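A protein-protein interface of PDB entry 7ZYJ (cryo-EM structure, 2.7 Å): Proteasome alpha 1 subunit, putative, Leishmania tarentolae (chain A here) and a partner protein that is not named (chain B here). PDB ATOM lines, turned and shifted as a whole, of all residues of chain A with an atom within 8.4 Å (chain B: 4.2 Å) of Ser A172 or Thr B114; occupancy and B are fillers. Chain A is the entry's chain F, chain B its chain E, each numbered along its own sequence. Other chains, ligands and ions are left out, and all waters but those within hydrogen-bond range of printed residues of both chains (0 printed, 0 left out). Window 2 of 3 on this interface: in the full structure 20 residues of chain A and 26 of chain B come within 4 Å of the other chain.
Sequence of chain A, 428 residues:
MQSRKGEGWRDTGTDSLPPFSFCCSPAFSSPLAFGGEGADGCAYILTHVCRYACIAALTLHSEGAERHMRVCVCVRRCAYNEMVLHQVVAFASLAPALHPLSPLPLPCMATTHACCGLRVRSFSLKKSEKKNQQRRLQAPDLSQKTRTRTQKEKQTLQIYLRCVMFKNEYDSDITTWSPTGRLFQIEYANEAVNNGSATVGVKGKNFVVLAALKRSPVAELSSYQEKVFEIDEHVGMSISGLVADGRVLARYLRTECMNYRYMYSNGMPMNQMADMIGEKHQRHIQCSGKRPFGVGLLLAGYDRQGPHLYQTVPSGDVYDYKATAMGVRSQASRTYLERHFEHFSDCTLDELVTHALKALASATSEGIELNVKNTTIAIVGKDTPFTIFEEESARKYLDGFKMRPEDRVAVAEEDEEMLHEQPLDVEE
Of the 17 printed residues of chain A, 5 touch a printed residue of chain B. Hydrophobic or aromatic side chains of chain A within 4 Å of the printed part of chain B: Tyr A188 and Pro A292. Among the printed residues, 9 pairs touch across the chains. Among the printed residues, no Asp or Glu carboxylate lies within 4 Å of a Lys or Arg side-chain nitrogen of the other chain.
Of chain B, only Thr B114 comes within 4 Å of Ser A172. Of chain A, only Ser A172 (3.2 Å) and Gln A185 (3.4 Å) come within 4 Å of Thr B114. Printed residues of chain B within 4 Å of Arg A291: Asn B113 (3.3 Å), Phe B115 (3.7 Å) and Ile B121 (3.6 Å). Of the printed residues of chain B, Pro A292 touches Phe B115. Of the printed residues of chain A, Asn B113 touches Arg A291 (3.3 Å). The nearest printed residue of chain B that does not touch Ser A172 is Arg B110 (4.6 Å).
N of Phe B115 is in hydrogen-bond range of OE1 of Gln A185.
OG1 of Thr B114 lies within hydrogen-bond range of O of Gly B111 (3.0 Å). O of Asp A171 is in hydrogen-bond range of NE2 of Gln A185, at 2.6 Å. The side-chain carboxylate (OD2) of Asp A171 is in hydrogen-bond range of the side-chain hydroxyl (OH) of Tyr A188 (2.9 Å).
Among the printed residues, merely in contact across the chains: Ser A172 with Thr B114, Gln A185 with Thr B114, Tyr A188 with Phe B115, Tyr A188 with Ser B116, Arg A291 with Asn B113, Arg A291 with Phe B115, Arg A291 with Ile B121 and Pro A292 with Phe B115.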
ATOM      1  N   ASN A 168     -15.258  -7.726   5.815  1.00  0.00           N
ATOM      2  CA  ASN A 168     -15.498  -6.321   5.510  1.00  0.00           C
ATOM      3  C   ASN A 168     -16.888  -5.898   5.971  1.00  0.00           C
ATOM      4  O   ASN A 168     -17.894  -6.424   5.500  1.00  0.00           O
ATOM      5  CB  ASN A 168     -15.337  -6.061   4.011  1.00  0.00           C
ATOM      6  CG  ASN A 168     -15.115  -4.597   3.693  1.00  0.00           C
ATOM      7  OD1 ASN A 168     -15.132  -3.747   4.584  1.00  0.00           O
ATOM      8  ND2 ASN A 168     -14.906  -4.293   2.419  1.00  0.00           N
ATOM      9  N   GLU A 169     -16.937  -4.939   6.897  1.00  0.00           N
ATOM     10  CA  GLU A 169     -18.194  -4.452   7.452  1.00  0.00           C
ATOM     11  C   GLU A 169     -18.534  -3.050   6.959  1.00  0.00           C
ATOM     12  O   GLU A 169     -19.368  -2.369   7.563  1.00  0.00           O
ATOM     13  CB  GLU A 169     -18.149  -4.478   8.982  1.00  0.00           C
ATOM     14  CG  GLU A 169     -16.988  -3.707   9.584  1.00  0.00           C
ATOM     15  CD  GLU A 169     -15.743  -4.557   9.742  1.00  0.00           C
ATOM     16  OE1 GLU A 169     -15.754  -5.720   9.288  1.00  0.00           O
ATOM     17  OE2 GLU A 169     -14.753  -4.062  10.321  1.00  0.00           O
ATOM     18  N   TYR A 170     -17.904  -2.604   5.871  1.00  0.00           N
ATOM     19  CA  TYR A 170     -18.157  -1.284   5.305  1.00  0.00           C
ATOM     20  C   TYR A 170     -18.591  -1.361   3.846  1.00  0.00           C
ATOM     21  O   TYR A 170     -18.601  -0.341   3.151  1.00  0.00           O
ATOM     22  CB  TYR A 170     -16.917  -0.400   5.442  1.00  0.00           C
ATOM     23  CG  TYR A 170     -16.504  -0.144   6.873  1.00  0.00           C
ATOM     24  CD1 TYR A 170     -17.088   0.875   7.613  1.00  0.00           C
ATOM     25  CD2 TYR A 170     -15.534  -0.925   7.485  1.00  0.00           C
ATOM     26  CE1 TYR A 170     -16.716   1.111   8.919  1.00  0.00           C
ATOM     27  CE2 TYR A 170     -15.156  -0.697   8.793  1.00  0.00           C
ATOM     28  CZ  TYR A 170     -15.749   0.321   9.505  1.00  0.00           C
ATOM     29  OH  TYR A 170     -15.376   0.554  10.809  1.00  0.00           O
ATOM     30  N   ASP A 171     -18.952  -2.551   3.368  1.00  0.00           N
ATOM     31  CA  ASP A 171     -19.337  -2.746   1.978  1.00  0.00           C
ATOM     32  C   ASP A 171     -20.805  -3.101   1.798  1.00  0.00           C
ATOM     33  O   ASP A 171     -21.248  -3.274   0.656  1.00  0.00           O
ATOM     34  CB  ASP A 171     -18.469  -3.836   1.335  1.00  0.00           C
ATOM     35  CG  ASP A 171     -18.527  -5.150   2.087  1.00  0.00           C
ATOM     36  OD1 ASP A 171     -19.183  -5.208   3.149  1.00  0.00           O
ATOM     37  OD2 ASP A 171     -17.916  -6.130   1.615  1.00  0.00           O
ATOM     38  N   SER A 172     -21.574  -3.216   2.880  1.00  0.00           N
ATOM     39  CA  SER A 172     -22.961  -3.645   2.781  1.00  0.00           C
ATOM     40  C   SER A 172     -23.931  -2.504   2.510  1.00  0.00           C
ATOM     41  O   SER A 172     -25.109  -2.767   2.249  1.00  0.00           O
ATOM     42  CB  SER A 172     -23.378  -4.369   4.063  1.00  0.00           C
ATOM     43  OG  SER A 172     -23.406  -3.478   5.165  1.00  0.00           O
ATOM     44  N   ASP A 173     -23.481  -1.252   2.565  1.00  0.00           N
ATOM     45  CA  ASP A 173     -24.367  -0.117   2.366  1.00  0.00           C
ATOM     46  C   ASP A 173     -23.691   0.912   1.472  1.00  0.00           C
ATOM     47  O   ASP A 173     -22.462   1.002   1.409  1.00  0.00           O
ATOM     48  CB  ASP A 173     -24.769   0.523   3.702  1.00  0.00           C
ATOM     49  CG  ASP A 173     -26.099   1.247   3.623  1.00  0.00           C
ATOM     50  OD1 ASP A 173     -26.535   1.575   2.500  1.00  0.00           O
ATOM     51  OD2 ASP A 173     -26.710   1.484   4.686  1.00  0.00           O
ATOM     52  N   ILE A 174     -24.518   1.692   0.776  1.00  0.00           N
ATOM     53  CA  ILE A 174     -24.012   2.759  -0.079  1.00  0.00           C
ATOM     54  C   ILE A 174     -23.688   4.037   0.688  1.00  0.00           C
ATOM     55  O   ILE A 174     -22.837   4.817   0.238  1.00  0.00           O
ATOM     56  CB  ILE A 174     -25.009   3.070  -1.212  1.00  0.00           C
ATOM     57  CG1 ILE A 174     -24.289   3.719  -2.392  1.00  0.00           C
ATOM     58  CG2 ILE A 174     -26.154   3.939  -0.721  1.00  0.00           C
ATOM     59  CD1 ILE A 174     -25.049   3.631  -3.673  1.00  0.00           C
ATOM     60  N   THR A 175     -24.334   4.275   1.831  1.00  0.00           N
ATOM     61  CA  THR A 175     -24.096   5.469   2.630  1.00  0.00           C
ATOM     62  C   THR A 175     -23.077   5.228   3.736  1.00  0.00           C
ATOM     63  O   THR A 175     -23.090   5.924   4.755  1.00  0.00           O
ATOM     64  CB  THR A 175     -25.407   5.984   3.225  1.00  0.00           C
ATOM     65  OG1 THR A 175     -25.944   5.005   4.124  1.00  0.00           O
ATOM     66  CG2 THR A 175     -26.415   6.271   2.127  1.00  0.00           C
ATOM     67  N   THR A 176     -22.193   4.252   3.553  1.00  0.00           N
ATOM     68  CA  THR A 176     -21.172   3.917   4.537  1.00  0.00           C
ATOM     69  C   THR A 176     -19.805   4.213   3.942  1.00  0.00           C
ATOM     70  O   THR A 176     -19.455   3.678   2.884  1.00  0.00           O
ATOM     71  CB  THR A 176     -21.268   2.450   4.956  1.00  0.00           C
ATOM     72  OG1 THR A 176     -22.540   2.208   5.569  1.00  0.00           O
ATOM     73  CG2 THR A 176     -20.164   2.106   5.944  1.00  0.00           C
ATOM     74  N   PHE A 184     -17.337   1.103  -1.085  1.00  0.00           N
ATOM     75  CA  PHE A 184     -17.123  -0.216  -1.669  1.00  0.00           C
ATOM     76  C   PHE A 184     -18.252  -0.628  -2.607  1.00  0.00           C
ATOM     77  O   PHE A 184     -18.021  -1.410  -3.534  1.00  0.00           O
ATOM     78  CB  PHE A 184     -16.946  -1.251  -0.561  1.00  0.00           C
ATOM     79  CG  PHE A 184     -15.544  -1.334  -0.035  1.00  0.00           C
ATOM     80  CD1 PHE A 184     -14.511  -1.773  -0.845  1.00  0.00           C
ATOM     81  CD2 PHE A 184     -15.256  -0.964   1.267  1.00  0.00           C
ATOM     82  CE1 PHE A 184     -13.218  -1.848  -0.364  1.00  0.00           C
ATOM     83  CE2 PHE A 184     -13.965  -1.036   1.753  1.00  0.00           C
ATOM     84  CZ  PHE A 184     -12.945  -1.477   0.936  1.00  0.00           C
ATOM     85  N   GLN A 185     -19.472  -0.136  -2.383  1.00  0.00           N
ATOM     86  CA  GLN A 185     -20.580  -0.491  -3.268  1.00  0.00           C
ATOM     87  C   GLN A 185     -20.353   0.042  -4.678  1.00  0.00           C
ATOM     88  O   GLN A 185     -20.615  -0.653  -5.668  1.00  0.00           O
ATOM     89  CB  GLN A 185     -21.896   0.034  -2.696  1.00  0.00           C
ATOM     90  CG  GLN A 185     -22.471  -0.831  -1.585  1.00  0.00           C
ATOM     91  CD  GLN A 185     -23.022  -2.148  -2.095  1.00  0.00           C
ATOM     92  OE1 GLN A 185     -23.993  -2.176  -2.851  1.00  0.00           O
ATOM     93  NE2 GLN A 185     -22.400  -3.247  -1.687  1.00  0.00           N
ATOM     94  N   TYR A 188     -17.839  -2.125  -6.314  1.00  0.00           N
ATOM     95  CA  TYR A 188     -18.474  -3.351  -6.784  1.00  0.00           C
ATOM     96  C   TYR A 188     -19.239  -3.115  -8.080  1.00  0.00           C
ATOM     97  O   TYR A 188     -19.244  -3.973  -8.969  1.00  0.00           O
ATOM     98  CB  TYR A 188     -19.403  -3.907  -5.705  1.00  0.00           C
ATOM     99  CG  TYR A 188     -18.693  -4.359  -4.447  1.00  0.00           C
ATOM    100  CD1 TYR A 188     -17.311  -4.500  -4.416  1.00  0.00           C
ATOM    101  CD2 TYR A 188     -19.404  -4.640  -3.290  1.00  0.00           C
ATOM    102  CE1 TYR A 188     -16.660  -4.908  -3.270  1.00  0.00           C
ATOM    103  CE2 TYR A 188     -18.761  -5.052  -2.139  1.00  0.00           C
ATOM    104  CZ  TYR A 188     -17.389  -5.184  -2.135  1.00  0.00           C
ATOM    105  OH  TYR A 188     -16.743  -5.593  -0.993  1.00  0.00           O
ATOM    106  N   ALA A 189     -19.902  -1.963  -8.199  1.00  0.00           N
ATOM    107  CA  ALA A 189     -20.555  -1.619  -9.460  1.00  0.00           C
ATOM    108  C   ALA A 189     -19.543  -1.463 -10.592  1.00  0.00           C
ATOM    109  O   ALA A 189     -19.810  -1.877 -11.729  1.00  0.00           O
ATOM    110  CB  ALA A 189     -21.377  -0.343  -9.292  1.00  0.00           C
ATOM    111  N   SER A 288     -29.822   6.302   0.812  1.00  0.00           N
ATOM    112  CA  SER A 288     -29.806   4.966   1.399  1.00  0.00           C
ATOM    113  C   SER A 288     -30.642   3.988   0.581  1.00  0.00           C
ATOM    114  O   SER A 288     -30.249   2.831   0.393  1.00  0.00           O
ATOM    115  CB  SER A 288     -30.305   5.022   2.842  1.00  0.00           C
ATOM    116  OG  SER A 288     -30.341   3.729   3.420  1.00  0.00           O
ATOM    117  N   LYS A 290     -31.112   3.673  -2.523  1.00  0.00           N
ATOM    118  CA  LYS A 290     -30.710   3.676  -3.921  1.00  0.00           C
ATOM    119  C   LYS A 290     -29.440   2.855  -4.077  1.00  0.00           C
ATOM    120  O   LYS A 290     -28.724   2.581  -3.110  1.00  0.00           O
ATOM    121  CB  LYS A 290     -30.497   5.102  -4.442  1.00  0.00           C
ATOM    122  CG  LYS A 290     -31.780   5.883  -4.662  1.00  0.00           C
ATOM    123  CD  LYS A 290     -31.518   7.164  -5.435  1.00  0.00           C
ATOM    124  CE  LYS A 290     -32.800   7.951  -5.649  1.00  0.00           C
ATOM    125  NZ  LYS A 290     -32.545   9.255  -6.320  1.00  0.00           N
ATOM    126  N   ARG A 291     -29.166   2.457  -5.317  1.00  0.00           N
ATOM    127  CA  ARG A 291     -27.974   1.694  -5.648  1.00  0.00           C
ATOM    128  C   ARG A 291     -27.391   2.260  -6.931  1.00  0.00           C
ATOM    129  O   ARG A 291     -28.131   2.828  -7.744  1.00  0.00           O
ATOM    130  CB  ARG A 291     -28.291   0.198  -5.811  1.00  0.00           C
ATOM    131  CG  ARG A 291     -29.112  -0.145  -7.038  1.00  0.00           C
ATOM    132  CD  ARG A 291     -28.903  -1.593  -7.444  1.00  0.00           C
ATOM    133  NE  ARG A 291     -29.718  -1.963  -8.593  1.00  0.00           N
ATOM    134  CZ  ARG A 291     -29.388  -1.721  -9.854  1.00  0.00           C
ATOM    135  NH1 ARG A 291     -28.259  -1.105 -10.166  1.00  0.00           N
ATOM    136  NH2 ARG A 291     -30.210  -2.104 -10.825  1.00  0.00           N
ATOM    137  N   PRO A 292     -26.082   2.142  -7.137  1.00  0.00           N
ATOM    138  CA  PRO A 292     -25.483   2.703  -8.350  1.00  0.00           C
ATOM    139  C   PRO A 292     -25.851   1.883  -9.575  1.00  0.00           C
ATOM    140  O   PRO A 292     -26.175   0.695  -9.494  1.00  0.00           O
ATOM    141  CB  PRO A 292     -23.979   2.639  -8.069  1.00  0.00           C
ATOM    142  CG  PRO A 292     -23.827   1.514  -7.114  1.00  0.00           C
ATOM    143  CD  PRO A 292     -25.095   1.422  -6.314  1.00  0.00           C
ATOM    144  N   ARG B 110     -27.732  -8.111   4.496  1.00  0.00           N
ATOM    145  CA  ARG B 110     -27.557  -7.260   3.329  1.00  0.00           C
ATOM    146  C   ARG B 110     -28.901  -6.716   2.865  1.00  0.00           C
ATOM    147  O   ARG B 110     -29.947  -7.343   3.053  1.00  0.00           O
ATOM    148  CB  ARG B 110     -26.889  -8.027   2.187  1.00  0.00           C
ATOM    149  CG  ARG B 110     -25.373  -8.086   2.270  1.00  0.00           C
ATOM    150  CD  ARG B 110     -24.910  -9.271   3.097  1.00  0.00           C
ATOM    151  NE  ARG B 110     -25.187 -10.538   2.431  1.00  0.00           N
ATOM    152  CZ  ARG B 110     -24.329 -11.176   1.647  1.00  0.00           C
ATOM    153  NH1 ARG B 110     -23.119 -10.696   1.413  1.00  0.00           N
ATOM    154  NH2 ARG B 110     -24.694 -12.324   1.086  1.00  0.00           N
ATOM    155  N   GLY B 111     -28.864  -5.537   2.255  1.00  0.00           N
ATOM    156  CA  GLY B 111     -30.047  -4.960   1.659  1.00  0.00           C
ATOM    157  C   GLY B 111     -30.376  -5.617   0.331  1.00  0.00           C
ATOM    158  O   GLY B 111     -29.645  -6.457  -0.193  1.00  0.00           O
ATOM    159  N   VAL B 112     -31.519  -5.215  -0.224  1.00  0.00           N
ATOM    160  CA  VAL B 112     -31.974  -5.788  -1.486  1.00  0.00           C
ATOM    161  C   VAL B 112     -31.313  -5.144  -2.700  1.00  0.00           C
ATOM    162  O   VAL B 112     -31.377  -5.711  -3.800  1.00  0.00           O
ATOM    163  CB  VAL B 112     -33.504  -5.685  -1.613  1.00  0.00           C
ATOM    164  CG1 VAL B 112     -34.179  -6.523  -0.539  1.00  0.00           C
ATOM    165  CG2 VAL B 112     -33.948  -4.234  -1.520  1.00  0.00           C
ATOM    166  N   ASN B 113     -30.682  -3.981  -2.536  1.00  0.00           N
ATOM    167  CA  ASN B 113     -30.015  -3.284  -3.627  1.00  0.00           C
ATOM    168  C   ASN B 113     -28.498  -3.420  -3.566  1.00  0.00           C
ATOM    169  O   ASN B 113     -27.792  -2.742  -4.319  1.00  0.00           O
ATOM    170  CB  ASN B 113     -30.411  -1.807  -3.626  1.00  0.00           C
ATOM    171  CG  ASN B 113     -31.813  -1.580  -4.153  1.00  0.00           C
ATOM    172  OD1 ASN B 113     -32.235  -2.209  -5.123  1.00  0.00           O
ATOM    173  ND2 ASN B 113     -32.544  -0.673  -3.515  1.00  0.00           N
ATOM    174  N   THR B 114     -27.983  -4.277  -2.691  1.00  0.00           N
ATOM    175  CA  THR B 114     -26.546  -4.385  -2.495  1.00  0.00           C
ATOM    176  C   THR B 114     -25.887  -5.152  -3.634  1.00  0.00           C
ATOM    177  O   THR B 114     -26.493  -6.026  -4.261  1.00  0.00           O
ATOM    178  CB  THR B 114     -26.233  -5.073  -1.166  1.00  0.00           C
ATOM    179  OG1 THR B 114     -26.799  -6.388  -1.164  1.00  0.00           O
ATOM    180  CG2 THR B 114     -26.812  -4.278  -0.015  1.00  0.00           C
ATOM    181  N   PHE B 115     -24.628  -4.814  -3.893  1.00  0.00           N
ATOM    182  CA  PHE B 115     -23.825  -5.471  -4.913  1.00  0.00           C
ATOM    183  C   PHE B 115     -22.896  -6.491  -4.270  1.00  0.00           C
ATOM    184  O   PHE B 115     -22.353  -6.257  -3.186  1.00  0.00           O
ATOM    185  CB  PHE B 115     -22.997  -4.452  -5.699  1.00  0.00           C
ATOM    186  CG  PHE B 115     -23.735  -3.811  -6.836  1.00  0.00           C
ATOM    187  CD1 PHE B 115     -23.829  -4.445  -8.063  1.00  0.00           C
ATOM    188  CD2 PHE B 115     -24.321  -2.565  -6.686  1.00  0.00           C
ATOM    189  CE1 PHE B 115     -24.501  -3.854  -9.114  1.00  0.00           C
ATOM    190  CE2 PHE B 115     -24.995  -1.970  -7.732  1.00  0.00           C
ATOM    191  CZ  PHE B 115     -25.085  -2.615  -8.949  1.00  0.00           C
ATOM    192  N   SER B 116     -22.721  -7.625  -4.941  1.00  0.00           N
ATOM    193  CA  SER B 116     -21.700  -8.575  -4.540  1.00  0.00           C
ATOM    194  C   SER B 116     -20.320  -8.022  -4.892  1.00  0.00           C
ATOM    195  O   SER B 116     -20.194  -7.176  -5.781  1.00  0.00           O
ATOM    196  CB  SER B 116     -21.924  -9.920  -5.232  1.00  0.00           C
ATOM    197  OG  SER B 116     -20.828 -10.799  -5.057  1.00  0.00           O
ATOM    198  N   ILE B 121     -25.918  -8.373  -8.240  1.00  0.00           N
ATOM    199  CA  ILE B 121     -26.906  -8.064  -7.215  1.00  0.00           C
ATOM    200  C   ILE B 121     -27.330  -9.356  -6.533  1.00  0.00           C
ATOM    201  O   ILE B 121     -27.693 -10.336  -7.193  1.00  0.00           O
ATOM    202  CB  ILE B 121     -28.107  -7.323  -7.827  1.00  0.00           C
ATOM    203  CG1 ILE B 121     -27.642  -6.025  -8.488  1.00  0.00           C
ATOM    204  CG2 ILE B 121     -29.158  -7.037  -6.767  1.00  0.00           C
ATOM    205  CD1 ILE B 121     -28.718  -5.316  -9.274  1.00  0.00           C
ATOM    206  N   PHE B 122     -27.274  -9.362  -5.199  1.00  0.00           N
ATOM    207  CA  PHE B 122     -27.514 -10.594  -4.450  1.00  0.00           C
ATOM    208  C   PHE B 122     -28.934 -11.109  -4.649  1.00  0.00           C
ATOM    209  O   PHE B 122     -29.139 -12.311  -4.847  1.00  0.00           O
ATOM    210  CB  PHE B 122     -27.234 -10.365  -2.965  1.00  0.00           C
ATOM    211  CG  PHE B 122     -25.781 -10.460  -2.601  1.00  0.00           C
ATOM    212  CD1 PHE B 122     -25.049 -11.594  -2.906  1.00  0.00           C
ATOM    213  CD2 PHE B 122     -25.148  -9.416  -1.949  1.00  0.00           C
ATOM    214  CE1 PHE B 122     -23.714 -11.685  -2.571  1.00  0.00           C
ATOM    215  CE2 PHE B 122     -23.813  -9.501  -1.611  1.00  0.00           C
ATOM    216  CZ  PHE B 122     -23.095 -10.636  -1.922  1.00  0.00           C
